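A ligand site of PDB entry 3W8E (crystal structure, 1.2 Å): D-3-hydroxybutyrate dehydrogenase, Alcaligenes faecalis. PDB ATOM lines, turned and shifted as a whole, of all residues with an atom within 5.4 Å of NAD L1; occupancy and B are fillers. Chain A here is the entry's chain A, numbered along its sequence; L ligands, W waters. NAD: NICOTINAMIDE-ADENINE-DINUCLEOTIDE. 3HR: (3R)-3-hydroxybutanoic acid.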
ATOM      1  N   GLY A  11      25.126 -17.364  -6.213  1.00  0.00           N
ATOM      2  CA  GLY A  11      24.067 -17.190  -7.219  1.00  0.00           C
ATOM      3  C   GLY A  11      24.136 -18.264  -8.241  1.00  0.00           C
ATOM      4  O   GLY A  11      24.016 -17.974  -9.444  1.00  0.00           O
ATOM      5  N   SER A  12      24.216 -19.501  -7.830  1.00  0.00           N
ATOM      6  CA  SER A  12      24.391 -20.686  -8.657  1.00  0.00           C
ATOM      7  C   SER A  12      23.178 -21.612  -8.621  1.00  0.00           C
ATOM      8  O   SER A  12      23.273 -22.713  -9.162  1.00  0.00           O
ATOM      9  CB  SER A  12      25.626 -21.465  -8.289  1.00  0.00           C
ATOM     10  OG  SER A  12      25.665 -21.586  -6.848  1.00  0.00           O
ATOM     11  N   THR A  13      22.043 -21.101  -8.214  1.00  0.00           N
ATOM     12  CA  THR A  13      20.804 -21.935  -8.330  1.00  0.00           C
ATOM     13  C   THR A  13      20.293 -21.876  -9.710  1.00  0.00           C
ATOM     14  O   THR A  13      19.481 -22.761 -10.041  1.00  0.00           O
ATOM     15  CB  THR A  13      19.790 -21.516  -7.266  1.00  0.00           C
ATOM     16  OG1 THR A  13      19.612 -20.104  -7.402  1.00  0.00           O
ATOM     17  CG2 THR A  13      20.276 -21.936  -5.905  1.00  0.00           C
ATOM     18  N   SER A  14      20.670 -20.881 -10.512  1.00  0.00           N
ATOM     19  CA  SER A  14      20.187 -20.807 -11.885  1.00  0.00           C
ATOM     20  C   SER A  14      21.148 -19.926 -12.719  1.00  0.00           C
ATOM     21  O   SER A  14      22.156 -19.442 -12.206  1.00  0.00           O
ATOM     22  CB  SER A  14      18.722 -20.477 -11.904  1.00  0.00           C
ATOM     23  OG  SER A  14      18.580 -19.242 -11.237  1.00  0.00           O
ATOM     24  N   GLY A  15      20.868 -19.850 -14.011  1.00  0.00           N
ATOM     25  CA  GLY A  15      21.649 -18.900 -14.836  1.00  0.00           C
ATOM     26  C   GLY A  15      23.073 -19.280 -15.016  1.00  0.00           C
ATOM     27  O   GLY A  15      23.472 -20.457 -15.064  1.00  0.00           O
ATOM     28  N   ILE A  16      23.863 -18.225 -15.151  1.00  0.00           N
ATOM     29  CA  ILE A  16      25.272 -18.414 -15.327  1.00  0.00           C
ATOM     30  C   ILE A  16      25.946 -19.164 -14.192  1.00  0.00           C
ATOM     31  O   ILE A  16      26.797 -19.996 -14.423  1.00  0.00           O
ATOM     32  CB  ILE A  16      25.949 -17.056 -15.562  1.00  0.00           C
ATOM     33  CG1 ILE A  16      25.437 -16.417 -16.877  1.00  0.00           C
ATOM     34  CG2 ILE A  16      27.446 -17.167 -15.482  1.00  0.00           C
ATOM     35  CD1 ILE A  16      25.865 -14.920 -16.981  1.00  0.00           C
ATOM     36  N   GLY A  17      25.540 -18.816 -12.973  1.00  0.00           N
ATOM     37  CA  GLY A  17      26.160 -19.489 -11.851  1.00  0.00           C
ATOM     38  C   GLY A  17      25.992 -20.976 -11.786  1.00  0.00           C
ATOM     39  O   GLY A  17      26.886 -21.660 -11.400  1.00  0.00           O
ATOM     40  N   ASN A  34      24.454 -21.708  -4.061  1.00  0.00           N
ATOM     41  CA  ASN A  34      23.874 -20.591  -3.309  1.00  0.00           C
ATOM     42  C   ASN A  34      22.868 -19.894  -4.152  1.00  0.00           C
ATOM     43  O   ASN A  34      23.022 -19.870  -5.373  1.00  0.00           O
ATOM     44  CB  ASN A  34      25.045 -19.673  -2.850  1.00  0.00           C
ATOM     45  CG  ASN A  34      24.593 -18.306  -2.471  1.00  0.00           C
ATOM     46  OD1 ASN A  34      24.595 -17.351  -3.266  1.00  0.00           O
ATOM     47  ND2 ASN A  34      24.132 -18.171  -1.218  1.00  0.00           N
ATOM     48  N   GLY A  35      21.866 -19.290  -3.578  1.00  0.00           N
ATOM     49  CA  GLY A  35      20.958 -18.472  -4.302  1.00  0.00           C
ATOM     50  C   GLY A  35      19.509 -18.821  -3.987  1.00  0.00           C
ATOM     51  O   GLY A  35      19.235 -19.652  -3.100  1.00  0.00           O
ATOM     52  N   PHE A  36      18.614 -18.187  -4.655  1.00  0.00           N
ATOM     53  CA  PHE A  36      17.156 -18.302  -4.344  1.00  0.00           C
ATOM     54  C   PHE A  36      16.578 -19.241  -5.354  1.00  0.00           C
ATOM     55  O   PHE A  36      17.136 -19.658  -6.321  1.00  0.00           O
ATOM     56  CB  PHE A  36      16.552 -16.937  -4.364  1.00  0.00           C
ATOM     57  CG  PHE A  36      17.085 -15.984  -3.362  1.00  0.00           C
ATOM     58  CD1 PHE A  36      17.345 -14.659  -3.766  1.00  0.00           C
ATOM     59  CD2 PHE A  36      17.518 -16.391  -2.124  1.00  0.00           C
ATOM     60  CE1 PHE A  36      17.807 -13.707  -2.887  1.00  0.00           C
ATOM     61  CE2 PHE A  36      18.148 -15.402  -1.200  1.00  0.00           C
ATOM     62  CZ  PHE A  36      18.218 -14.071  -1.616  1.00  0.00           C
ATOM     63  N   GLY A  37      15.301 -19.630  -5.114  1.00  0.00           N
ATOM     64  CA  GLY A  37      14.566 -20.486  -6.049  1.00  0.00           C
ATOM     65  C   GLY A  37      13.670 -21.451  -5.232  1.00  0.00           C
ATOM     66  O   GLY A  37      13.666 -21.438  -3.966  1.00  0.00           O
ATOM     67  N   ALA A  62      22.114 -17.970   1.570  1.00  0.00           N
ATOM     68  CA  ALA A  62      22.508 -16.714   2.185  1.00  0.00           C
ATOM     69  C   ALA A  62      22.075 -15.601   1.307  1.00  0.00           C
ATOM     70  O   ALA A  62      22.293 -15.704   0.069  1.00  0.00           O
ATOM     71  CB  ALA A  62      24.068 -16.669   2.445  1.00  0.00           C
ATOM     72  N   ASP A  63      21.523 -14.519   1.809  1.00  0.00           N
ATOM     73  CA  ASP A  63      21.176 -13.369   1.041  1.00  0.00           C
ATOM     74  C   ASP A  63      22.421 -12.549   1.124  1.00  0.00           C
ATOM     75  O   ASP A  63      22.783 -11.896   2.127  1.00  0.00           O
ATOM     76  CB  ASP A  63      19.948 -12.648   1.653  1.00  0.00           C
ATOM     77  CG  ASP A  63      19.635 -11.420   0.872  1.00  0.00           C
ATOM     78  OD1 ASP A  63      18.516 -10.846   1.170  1.00  0.00           O
ATOM     79  OD2 ASP A  63      20.381 -10.838   0.129  1.00  0.00           O
ATOM     80  N   LEU A  64      23.112 -12.456  -0.015  1.00  0.00           N
ATOM     81  CA  LEU A  64      24.473 -11.818  -0.023  1.00  0.00           C
ATOM     82  C   LEU A  64      24.357 -10.313  -0.115  1.00  0.00           C
ATOM     83  O   LEU A  64      25.401  -9.637  -0.137  1.00  0.00           O
ATOM     84  CB  LEU A  64      25.240 -12.382  -1.175  1.00  0.00           C
ATOM     85  CG  LEU A  64      25.350 -13.915  -1.100  1.00  0.00           C
ATOM     86  CD1 LEU A  64      26.139 -14.400  -2.346  1.00  0.00           C
ATOM     87  CD2 LEU A  64      26.102 -14.374   0.177  1.00  0.00           C
ATOM     88  N   SER A  65      23.190  -9.711  -0.070  1.00  0.00           N
ATOM     89  CA  SER A  65      23.158  -8.269   0.102  1.00  0.00           C
ATOM     90  C   SER A  65      23.473  -7.786   1.497  1.00  0.00           C
ATOM     91  O   SER A  65      23.525  -6.576   1.714  1.00  0.00           O
ATOM     92  CB  SER A  65      21.799  -7.739  -0.268  1.00  0.00           C
ATOM     93  OG  SER A  65      20.788  -8.218   0.595  1.00  0.00           O
ATOM     94  N   ASN A  90      29.376 -14.422  -8.404  1.00  0.00           N
ATOM     95  CA  ASN A  90      28.479 -14.346  -9.542  1.00  0.00           C
ATOM     96  C   ASN A  90      27.140 -13.725  -9.263  1.00  0.00           C
ATOM     97  O   ASN A  90      26.573 -13.080 -10.166  1.00  0.00           O
ATOM     98  CB  ASN A  90      28.295 -15.741 -10.085  1.00  0.00           C
ATOM     99  CG  ASN A  90      27.181 -15.851 -11.058  1.00  0.00           C
ATOM    100  OD1 ASN A  90      27.309 -15.552 -12.283  1.00  0.00           O
ATOM    101  ND2 ASN A  90      26.040 -16.303 -10.578  1.00  0.00           N
ATOM    102  N   ALA A  91      26.577 -13.867  -8.097  1.00  0.00           N
ATOM    103  CA  ALA A  91      25.193 -13.415  -7.851  1.00  0.00           C
ATOM    104  C   ALA A  91      25.030 -11.946  -8.232  1.00  0.00           C
ATOM    105  O   ALA A  91      25.895 -11.102  -7.951  1.00  0.00           O
ATOM    106  CB  ALA A  91      24.916 -13.575  -6.339  1.00  0.00           C
ATOM    107  N   GLY A  92      23.937 -11.590  -8.895  1.00  0.00           N
ATOM    108  CA  GLY A  92      23.717 -10.192  -9.292  1.00  0.00           C
ATOM    109  C   GLY A  92      22.269 -10.016  -9.679  1.00  0.00           C
ATOM    110  O   GLY A  92      21.596 -11.006 -10.072  1.00  0.00           O
ATOM    111  N   ILE A  93      21.857  -8.748  -9.676  1.00  0.00           N
ATOM    112  CA  ILE A  93      20.504  -8.338 -10.116  1.00  0.00           C
ATOM    113  C   ILE A  93      20.647  -7.141 -11.043  1.00  0.00           C
ATOM    114  O   ILE A  93      21.696  -6.479 -11.098  1.00  0.00           O
ATOM    115  CB  ILE A  93      19.561  -8.032  -8.955  1.00  0.00           C
ATOM    116  CG1 ILE A  93      20.242  -7.007  -8.044  1.00  0.00           C
ATOM    117  CG2 ILE A  93      19.269  -9.358  -8.134  1.00  0.00           C
ATOM    118  CD1 ILE A  93      19.290  -6.424  -6.984  1.00  0.00           C
ATOM    119  N   LEU A 113      24.520  -6.079  -3.672  1.00  0.00           N
ATOM    120  CA  LEU A 113      24.722  -7.441  -4.177  1.00  0.00           C
ATOM    121  C   LEU A 113      25.842  -7.471  -5.212  1.00  0.00           C
ATOM    122  O   LEU A 113      26.712  -8.317  -5.174  1.00  0.00           O
ATOM    123  CB  LEU A 113      23.438  -8.035  -4.749  1.00  0.00           C
ATOM    124  CG  LEU A 113      23.612  -9.482  -5.262  1.00  0.00           C
ATOM    125  CD1 LEU A 113      24.005 -10.441  -4.106  1.00  0.00           C
ATOM    126  CD2 LEU A 113      22.373  -9.976  -5.924  1.00  0.00           C
ATOM    127  N   ASN A 114      25.728  -6.594  -6.199  1.00  0.00           N
ATOM    128  CA  ASN A 114      26.640  -6.682  -7.356  1.00  0.00           C
ATOM    129  C   ASN A 114      28.022  -6.151  -7.033  1.00  0.00           C
ATOM    130  O   ASN A 114      28.945  -6.493  -7.782  1.00  0.00           O
ATOM    131  CB  ASN A 114      26.047  -5.924  -8.568  1.00  0.00           C
ATOM    132  CG  ASN A 114      24.763  -6.496  -9.079  1.00  0.00           C
ATOM    133  OD1 ASN A 114      23.972  -7.177  -8.418  1.00  0.00           O
ATOM    134  ND2 ASN A 114      24.452  -6.194 -10.355  1.00  0.00           N
ATOM    135  N   ILE A 140      32.339 -12.194 -11.670  1.00  0.00           N
ATOM    136  CA  ILE A 140      31.528 -12.061 -12.881  1.00  0.00           C
ATOM    137  C   ILE A 140      31.114 -10.644 -12.939  1.00  0.00           C
ATOM    138  O   ILE A 140      30.195 -10.181 -12.235  1.00  0.00           O
ATOM    139  CB  ILE A 140      30.320 -13.014 -12.903  1.00  0.00           C
ATOM    140  CG1 ILE A 140      30.748 -14.474 -12.617  1.00  0.00           C
ATOM    141  CG2 ILE A 140      29.577 -12.852 -14.262  1.00  0.00           C
ATOM    142  CD1 ILE A 140      31.875 -15.019 -13.494  1.00  0.00           C
ATOM    143  N   ALA A 141      31.775  -9.879 -13.812  1.00  0.00           N
ATOM    144  CA  ALA A 141      31.482  -8.517 -14.066  1.00  0.00           C
ATOM    145  C   ALA A 141      30.596  -8.462 -15.257  1.00  0.00           C
ATOM    146  O   ALA A 141      29.483  -9.069 -15.161  1.00  0.00           O
ATOM    147  CB  ALA A 141      32.712  -7.605 -14.175  1.00  0.00           C
ATOM    148  N   SER A 142      30.899  -7.737 -16.319  1.00  0.00           N
ATOM    149  CA  SER A 142      30.030  -7.568 -17.510  1.00  0.00           C
ATOM    150  C   SER A 142      30.800  -6.717 -18.465  1.00  0.00           C
ATOM    151  O   SER A 142      31.724  -6.015 -18.095  1.00  0.00           O
ATOM    152  CB  SER A 142      28.776  -6.748 -17.061  1.00  0.00           C
ATOM    153  OG  SER A 142      28.010  -6.473 -18.215  1.00  0.00           O
ATOM    154  N   ALA A 143      30.347  -6.714 -19.757  1.00  0.00           N
ATOM    155  CA  ALA A 143      30.757  -5.648 -20.632  1.00  0.00           C
ATOM    156  C   ALA A 143      30.458  -4.287 -19.988  1.00  0.00           C
ATOM    157  O   ALA A 143      31.219  -3.317 -20.180  1.00  0.00           O
ATOM    158  CB  ALA A 143      30.035  -5.803 -21.930  1.00  0.00           C
ATOM    159  N   TYR A 155      23.830  -0.577 -12.155  1.00  0.00           N
ATOM    160  CA  TYR A 155      24.528  -1.786 -12.593  1.00  0.00           C
ATOM    161  C   TYR A 155      25.907  -1.501 -13.214  1.00  0.00           C
ATOM    162  O   TYR A 155      26.851  -2.177 -12.938  1.00  0.00           O
ATOM    163  CB  TYR A 155      23.623  -2.488 -13.584  1.00  0.00           C
ATOM    164  CG  TYR A 155      24.073  -3.812 -14.086  1.00  0.00           C
ATOM    165  CD1 TYR A 155      24.865  -3.950 -15.230  1.00  0.00           C
ATOM    166  CD2 TYR A 155      23.640  -4.977 -13.448  1.00  0.00           C
ATOM    167  CE1 TYR A 155      25.205  -5.226 -15.735  1.00  0.00           C
ATOM    168  CE2 TYR A 155      24.009  -6.238 -13.896  1.00  0.00           C
ATOM    169  CZ  TYR A 155      24.747  -6.335 -15.113  1.00  0.00           C
ATOM    170  OH  TYR A 155      25.110  -7.554 -15.602  1.00  0.00           O
ATOM    171  N   LYS A 159      29.348  -2.751 -11.701  1.00  0.00           N
ATOM    172  CA  LYS A 159      30.225  -3.646 -12.474  1.00  0.00           C
ATOM    173  C   LYS A 159      31.561  -2.966 -12.719  1.00  0.00           C
ATOM    174  O   LYS A 159      32.602  -3.641 -12.705  1.00  0.00           O
ATOM    175  CB  LYS A 159      29.575  -4.055 -13.797  1.00  0.00           C
ATOM    176  CG  LYS A 159      28.384  -4.938 -13.624  1.00  0.00           C
ATOM    177  CD  LYS A 159      28.675  -6.258 -12.920  1.00  0.00           C
ATOM    178  CE  LYS A 159      27.495  -7.205 -12.995  1.00  0.00           C
ATOM    179  NZ  LYS A 159      27.825  -8.489 -12.386  1.00  0.00           N
ATOM    180  N   PRO A 185      31.070 -10.815 -19.508  1.00  0.00           N
ATOM    181  CA  PRO A 185      30.208 -11.297 -20.625  1.00  0.00           C
ATOM    182  C   PRO A 185      29.447 -10.209 -21.244  1.00  0.00           C
ATOM    183  O   PRO A 185      29.088  -9.216 -20.609  1.00  0.00           O
ATOM    184  CB  PRO A 185      29.259 -12.313 -19.943  1.00  0.00           C
ATOM    185  CG  PRO A 185      29.899 -12.561 -18.608  1.00  0.00           C
ATOM    186  CD  PRO A 185      30.546 -11.282 -18.194  1.00  0.00           C
ATOM    187  N   GLY A 186      29.153 -10.402 -22.537  1.00  0.00           N
ATOM    188  CA  GLY A 186      28.055  -9.685 -23.211  1.00  0.00           C
ATOM    189  C   GLY A 186      26.766 -10.400 -22.923  1.00  0.00           C
ATOM    190  O   GLY A 186      26.630 -11.081 -21.877  1.00  0.00           O
ATOM    191  N   TRP A 187      25.766 -10.283 -23.765  1.00  0.00           N
ATOM    192  CA  TRP A 187      24.446 -10.835 -23.497  1.00  0.00           C
ATOM    193  C   TRP A 187      24.451 -12.306 -23.457  1.00  0.00           C
ATOM    194  O   TRP A 187      25.001 -12.971 -24.396  1.00  0.00           O
ATOM    195  CB  TRP A 187      23.482 -10.435 -24.593  1.00  0.00           C
ATOM    196  CG  TRP A 187      23.188  -9.016 -24.798  1.00  0.00           C
ATOM    197  CD1 TRP A 187      23.312  -8.314 -25.986  1.00  0.00           C
ATOM    198  CD2 TRP A 187      22.514  -8.126 -23.907  1.00  0.00           C
ATOM    199  NE1 TRP A 187      22.819  -7.046 -25.843  1.00  0.00           N
ATOM    200  CE2 TRP A 187      22.317  -6.905 -24.595  1.00  0.00           C
ATOM    201  CE3 TRP A 187      22.096  -8.210 -22.578  1.00  0.00           C
ATOM    202  CZ2 TRP A 187      21.633  -5.838 -24.051  1.00  0.00           C
ATOM    203  CZ3 TRP A 187      21.376  -7.129 -22.083  1.00  0.00           C
ATOM    204  CH2 TRP A 187      21.232  -5.971 -22.758  1.00  0.00           C
ATOM    205  N   VAL A 188      23.846 -12.879 -22.433  1.00  0.00           N
ATOM    206  CA  VAL A 188      23.637 -14.261 -22.176  1.00  0.00           C
ATOM    207  C   VAL A 188      22.134 -14.454 -21.910  1.00  0.00           C
ATOM    208  O   VAL A 188      21.594 -13.712 -21.097  1.00  0.00           O
ATOM    209  CB  VAL A 188      24.436 -14.769 -20.928  1.00  0.00           C
ATOM    210  CG1 VAL A 188      24.263 -16.242 -20.732  1.00  0.00           C
ATOM    211  CG2 VAL A 188      25.863 -14.386 -21.026  1.00  0.00           C
ATOM    212  N   ARG A 189      21.470 -15.373 -22.588  1.00  0.00           N
ATOM    213  CA  ARG A 189      19.999 -15.411 -22.518  1.00  0.00           C
ATOM    214  C   ARG A 189      19.541 -16.195 -21.308  1.00  0.00           C
ATOM    215  O   ARG A 189      18.970 -17.297 -21.350  1.00  0.00           O
ATOM    216  CB  ARG A 189      19.419 -15.939 -23.805  1.00  0.00           C
ATOM    217  CG  ARG A 189      17.902 -15.567 -23.947  1.00  0.00           C
ATOM    218  CD  ARG A 189      17.437 -16.059 -25.263  1.00  0.00           C
ATOM    219  NE  ARG A 189      16.023 -15.629 -25.356  1.00  0.00           N
ATOM    220  CZ  ARG A 189      15.392 -15.600 -26.516  1.00  0.00           C
ATOM    221  NH1 ARG A 189      15.945 -16.109 -27.634  1.00  0.00           N
ATOM    222  NH2 ARG A 189      14.146 -15.154 -26.479  1.00  0.00           N
ATOM    223  N   THR A 190      19.692 -15.551 -20.112  1.00  0.00           N
ATOM    224  CA  THR A 190      19.156 -16.018 -18.831  1.00  0.00           C
ATOM    225  C   THR A 190      17.867 -15.184 -18.553  1.00  0.00           C
ATOM    226  O   THR A 190      17.512 -14.253 -19.244  1.00  0.00           O
ATOM    227  CB  THR A 190      20.176 -15.689 -17.714  1.00  0.00           C
ATOM    228  OG1 THR A 190      20.219 -14.289 -17.575  1.00  0.00           O
ATOM    229  CG2 THR A 190      21.553 -16.218 -18.062  1.00  0.00           C
ATOM    230  N   PRO A 191      17.202 -15.503 -17.422  1.00  0.00           N
ATOM    231  CA  PRO A 191      16.029 -14.696 -17.063  1.00  0.00           C
ATOM    232  C   PRO A 191      16.297 -13.251 -16.803  1.00  0.00           C
ATOM    233  O   PRO A 191      15.426 -12.447 -17.086  1.00  0.00           O
ATOM    234  CB  PRO A 191      15.489 -15.354 -15.787  1.00  0.00           C
ATOM    235  CG  PRO A 191      15.938 -16.813 -15.950  1.00  0.00           C
ATOM    236  CD  PRO A 191      17.376 -16.669 -16.530  1.00  0.00           C
ATOM    237  N   LEU A 192      17.554 -12.898 -16.459  1.00  0.00           N
ATOM    238  CA  LEU A 192      17.927 -11.515 -16.260  1.00  0.00           C
ATOM    239  C   LEU A 192      17.818 -10.723 -17.573  1.00  0.00           C
ATOM    240  O   LEU A 192      17.377  -9.582 -17.651  1.00  0.00           O
ATOM    241  CB  LEU A 192      19.339 -11.493 -15.676  1.00  0.00           C
ATOM    242  CG  LEU A 192      19.903 -10.073 -15.344  1.00  0.00           C
ATOM    243  CD1 LEU A 192      20.887 -10.134 -14.109  1.00  0.00           C
ATOM    244  CD2 LEU A 192      20.558  -9.470 -16.564  1.00  0.00           C
ATOM    245  N   VAL A 193      18.153 -11.376 -18.674  1.00  0.00           N
ATOM    246  CA  VAL A 193      18.052 -10.796 -20.020  1.00  0.00           C
ATOM    247  C   VAL A 193      16.682 -11.015 -20.661  1.00  0.00           C
ATOM    248  O   VAL A 193      16.200 -10.157 -21.368  1.00  0.00           O
ATOM    249  CB  VAL A 193      19.254 -11.340 -20.857  1.00  0.00           C
ATOM    250  CG1 VAL A 193      19.040 -11.080 -22.370  1.00  0.00           C
ATOM    251  CG2 VAL A 193      20.526 -10.697 -20.329  1.00  0.00           C
HETATM  252  PA  NAD L   1      20.004 -14.826 -13.046  1.00  0.00           P
HETATM  253  O1A NAD L   1      18.973 -13.826 -12.635  1.00  0.00           O
HETATM  254  O2A NAD L   1      19.634 -15.819 -14.033  1.00  0.00           O
HETATM  255  O5B NAD L   1      20.672 -15.519 -11.806  1.00  0.00           O
HETATM  256  C5B NAD L   1      21.005 -14.732 -10.603  1.00  0.00           C
HETATM  257  C4B NAD L   1      21.416 -15.754  -9.532  1.00  0.00           C
HETATM  258  O4B NAD L   1      21.714 -14.917  -8.366  1.00  0.00           O
HETATM  259  C3B NAD L   1      20.309 -16.714  -9.094  1.00  0.00           C
HETATM  260  O3B NAD L   1      20.914 -17.889  -8.596  1.00  0.00           O
HETATM  261  C2B NAD L   1      19.642 -15.902  -8.003  1.00  0.00           C
HETATM  262  O2B NAD L   1      18.889 -16.746  -7.085  1.00  0.00           O
HETATM  263  C1B NAD L   1      20.871 -15.394  -7.300  1.00  0.00           C
HETATM  264  N9A NAD L   1      20.696 -14.244  -6.412  1.00  0.00           N
HETATM  265  C8A NAD L   1      19.903 -13.128  -6.638  1.00  0.00           C
HETATM  266  N7A NAD L   1      19.872 -12.331  -5.556  1.00  0.00           N
HETATM  267  C5A NAD L   1      20.693 -12.959  -4.598  1.00  0.00           C
HETATM  268  C6A NAD L   1      20.997 -12.596  -3.297  1.00  0.00           C
HETATM  269  N6A NAD L   1      20.607 -11.448  -2.742  1.00  0.00           N
HETATM  270  N1A NAD L   1      21.836 -13.436  -2.682  1.00  0.00           N
HETATM  271  C2A NAD L   1      22.261 -14.569  -3.213  1.00  0.00           C
HETATM  272  N3A NAD L   1      21.969 -14.967  -4.469  1.00  0.00           N
HETATM  273  C4A NAD L   1      21.176 -14.134  -5.112  1.00  0.00           C
HETATM  274  O3  NAD L   1      21.192 -13.963 -13.649  1.00  0.00           O
HETATM  275  PN  NAD L   1      22.431 -14.267 -14.567  1.00  0.00           P
HETATM  276  O1N NAD L   1      22.110 -13.647 -15.920  1.00  0.00           O
HETATM  277  O2N NAD L   1      22.822 -15.649 -14.464  1.00  0.00           O
HETATM  278  O5D NAD L   1      23.562 -13.336 -13.952  1.00  0.00           O
HETATM  279  C5D NAD L   1      24.606 -13.869 -13.131  1.00  0.00           C
HETATM  280  C4D NAD L   1      25.669 -12.804 -13.075  1.00  0.00           C
HETATM  281  O4D NAD L   1      26.143 -12.585 -14.425  1.00  0.00           O
HETATM  282  C3D NAD L   1      25.190 -11.459 -12.520  1.00  0.00           C
HETATM  283  O3D NAD L   1      26.273 -10.896 -11.758  1.00  0.00           O
HETATM  284  C2D NAD L   1      25.034 -10.625 -13.792  1.00  0.00           C
HETATM  285  O2D NAD L   1      25.258  -9.308 -13.563  1.00  0.00           O
HETATM  286  C1D NAD L   1      26.150 -11.199 -14.603  1.00  0.00           C
HETATM  287  N1N NAD L   1      26.005 -10.966 -16.068  1.00  0.00           N
HETATM  288  C2N NAD L   1      24.961 -11.444 -16.764  1.00  0.00           C
HETATM  289  C3N NAD L   1      24.865 -11.288 -18.086  1.00  0.00           C
HETATM  290  C7N NAD L   1      23.785 -11.738 -18.880  1.00  0.00           C
HETATM  291  O7N NAD L   1      23.640 -11.278 -20.099  1.00  0.00           O
HETATM  292  N7N NAD L   1      22.839 -12.555 -18.426  1.00  0.00           N
HETATM  293  C4N NAD L   1      25.916 -10.646 -18.798  1.00  0.00           C
HETATM  294  C5N NAD L   1      27.041 -10.196 -18.070  1.00  0.00           C
HETATM  295  C6N NAD L   1      27.115 -10.359 -16.678  1.00  0.00           C
HETATM  296  C1  3HR L   2      22.694  -6.404 -18.608  1.00  0.00           C
HETATM  297  O1  3HR L   2      23.281  -5.350 -18.969  1.00  0.00           O
HETATM  298  C2  3HR L   2      23.332  -7.769 -18.735  1.00  0.00           C
HETATM  299  O2  3HR L   2      25.558  -7.143 -18.189  1.00  0.00           O
HETATM  300  C3  3HR L   2      24.780  -7.830 -19.140  1.00  0.00           C
HETATM  301  O3  3HR L   2      21.519  -6.389 -18.135  1.00  0.00           O
HETATM  302  C4  3HR L   2      25.083  -7.295 -20.534  1.00  0.00           C
HETATM  303  O   HOH W   1      19.062 -11.564 -11.041  1.00  0.00           O
HETATM  304  O   HOH W   2      16.463 -13.217 -13.223  1.00  0.00           O
HETATM  305  O   HOH W   3      17.559 -10.773  -5.181  1.00  0.00           O
HETATM  306  O   HOH W   4      16.471 -16.856  -8.139  1.00  0.00           O
HETATM  307  O   HOH W   5      17.702 -12.846  -9.062  1.00  0.00           O
HETATM  308  O   HOH W   6      23.635 -16.894 -12.164  1.00  0.00           O
HETATM  309  O   HOH W   7      18.061 -17.810 -13.270  1.00  0.00           O
HETATM  310  O   HOH W   8      19.043  -8.891  -3.555  1.00  0.00           O
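N of Val 188 is in hydrogen-bond range of O7N of NAD L1 (2.8 Å).
N of Phe 36 is in hydrogen-bond range of O2B of NAD L1, at 2.8 Å.
O2D of NAD L1 sits at hydrogen-bond distance from OH of Tyr 155 (2.7 Å).
The backbone NH (N) of Leu 64 is in hydrogen-bond range of a nitrogen (N1A) of NAD L1 (3.1 Å).
O of Val 188 sits at hydrogen-bond distance from N7N of NAD L1 (3.2 Å).
O3B of NAD L1 is in hydrogen-bond range of O of Gly 11 (3.2 Å).
NZ of Lys 159 is in hydrogen-bond range of O3D of NAD L1, 2.9 Å away.
N of Thr 13 sits at hydrogen-bond distance from O3B of NAD L1 (3.4 Å).
OG1 of Thr 190 sits at hydrogen-bond distance from O1N of NAD L1 (2.6 Å).
The side-chain carboxylate (OD2) of Asp 63 lies within hydrogen-bond range of a nitrogen (N6A) of NAD L1 (2.9 Å).
The side-chain hydroxyl (OG) of Ser 142 is in hydrogen-bond range of an oxygen (O2) of 3HR L2 (2.5 Å).
The backbone NH (N) of Ile 16 sits at hydrogen-bond distance from an oxygen (O2N) of NAD L1 (2.9 Å).
O of Asn 90 sits at hydrogen-bond distance from O3D of NAD L1 (2.7 Å).
The side-chain hydroxyl of Tyr 155 lies within hydrogen-bond range of an oxygen (O2) of 3HR L2 (2.7 Å).
The side-chain hydroxyl (OG1) of Thr 13 sits at hydrogen-bond distance from an oxygen (O3B) of NAD L1 (2.8 Å).
O of Phe 36 sits at hydrogen-bond distance from O2B of NAD L1, 3.5 Å away.
The backbone NH (N) of Thr 13 lies within hydrogen-bond range of the backbone carbonyl oxygen (O) of Asn 34 (3.2 Å).
The side-chain amide nitrogen (ND2) of Asn 34 lies within hydrogen-bond range of the backbone carbonyl oxygen (O) of Ala 62 (3.3 Å).
The backbone NH of Leu 192 sits close to the side-chain hydroxyl of Thr 190 (3.2 Å).
N of Gly 11 sits at hydrogen-bond distance from OD1 of Asn 34 (3.0 Å).
O of Ala 141 sits at hydrogen-bond distance from NZ of Lys 159 (3.3 Å).
The backbone carbonyl oxygen (O) of Ile 140 lies within hydrogen-bond range of the side-chain amino group (NZ) of Lys 159 (2.9 Å).
The backbone carbonyl oxygen (O) of Pro 185 sits at hydrogen-bond distance from the backbone NH (N) of Ala 143, 2.9 Å away.
O of Gly 11 is in hydrogen-bond range of ND2 of Asn 90.
The backbone carbonyl oxygen (O) of Gly 186 sits close to an oxygen (O7N) of NAD L1 (3.5 Å).
Merely in contact with NAD L1: Ala 141, Val 193, Pro 185, Ile 140, Leu 113, Pro 191, Ala 62, Gly 15, Leu 192, Trp 187, Ser 14, Gly 92, Asn 34, Gly 35, Ser 12, Ala 91, Ser 142 and Ile 93.
Hydrophobic or aromatic side chains that line NAD L1: Ile 16, Phe 36, Leu 64, Ala 91, Ile 93, Leu 113, Ile 140, Tyr 155, Pro 185, Val 188, Pro 191, Leu 192 and Val 193.
30 residues have an atom within 4 Å of NAD L1: Gly 11, Ser 12, Thr 13, Ser 14, Gly 15, Ile 16, Asn 34, Gly 35, Phe 36, Ala 62, Asp 63, Leu 64, Asn 90, Ala 91, Gly 92, Ile 93, Leu 113, Ile 140, Ala 141, Ser 142, Tyr 155, Lys 159, Pro 185, Gly 186, Trp 187, Val 188, Thr 190, Pro 191, Leu 192 and Val 193.
Along chain A the residues within 4 Å of NAD L1 span positions 11 to 193.
The nearest printed residue that does not touch NAD L1 is Ser 65 (4.1 Å).
Water W4 lies within hydrogen-bond range of an oxygen (O2B) of NAD L1 (2.6 Å) and the backbone carbonyl oxygen of Phe 36 (3.4 Å).
Water W2 lies within hydrogen-bond range of O1A of NAD L1 (2.6 Å) and N of Leu 192 (3.4 Å).
Water W7 lies within hydrogen-bond range of the side-chain hydroxyl of Ser 14 (2.5 Å) and an oxygen (O2A) of NAD L1 (2.6 Å).
Water W1 lies within hydrogen-bond range of an oxygen (O1A) of NAD L1 (2.8 Å) and the backbone carbonyl oxygen (O) of Gly 92 (2.8 Å).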
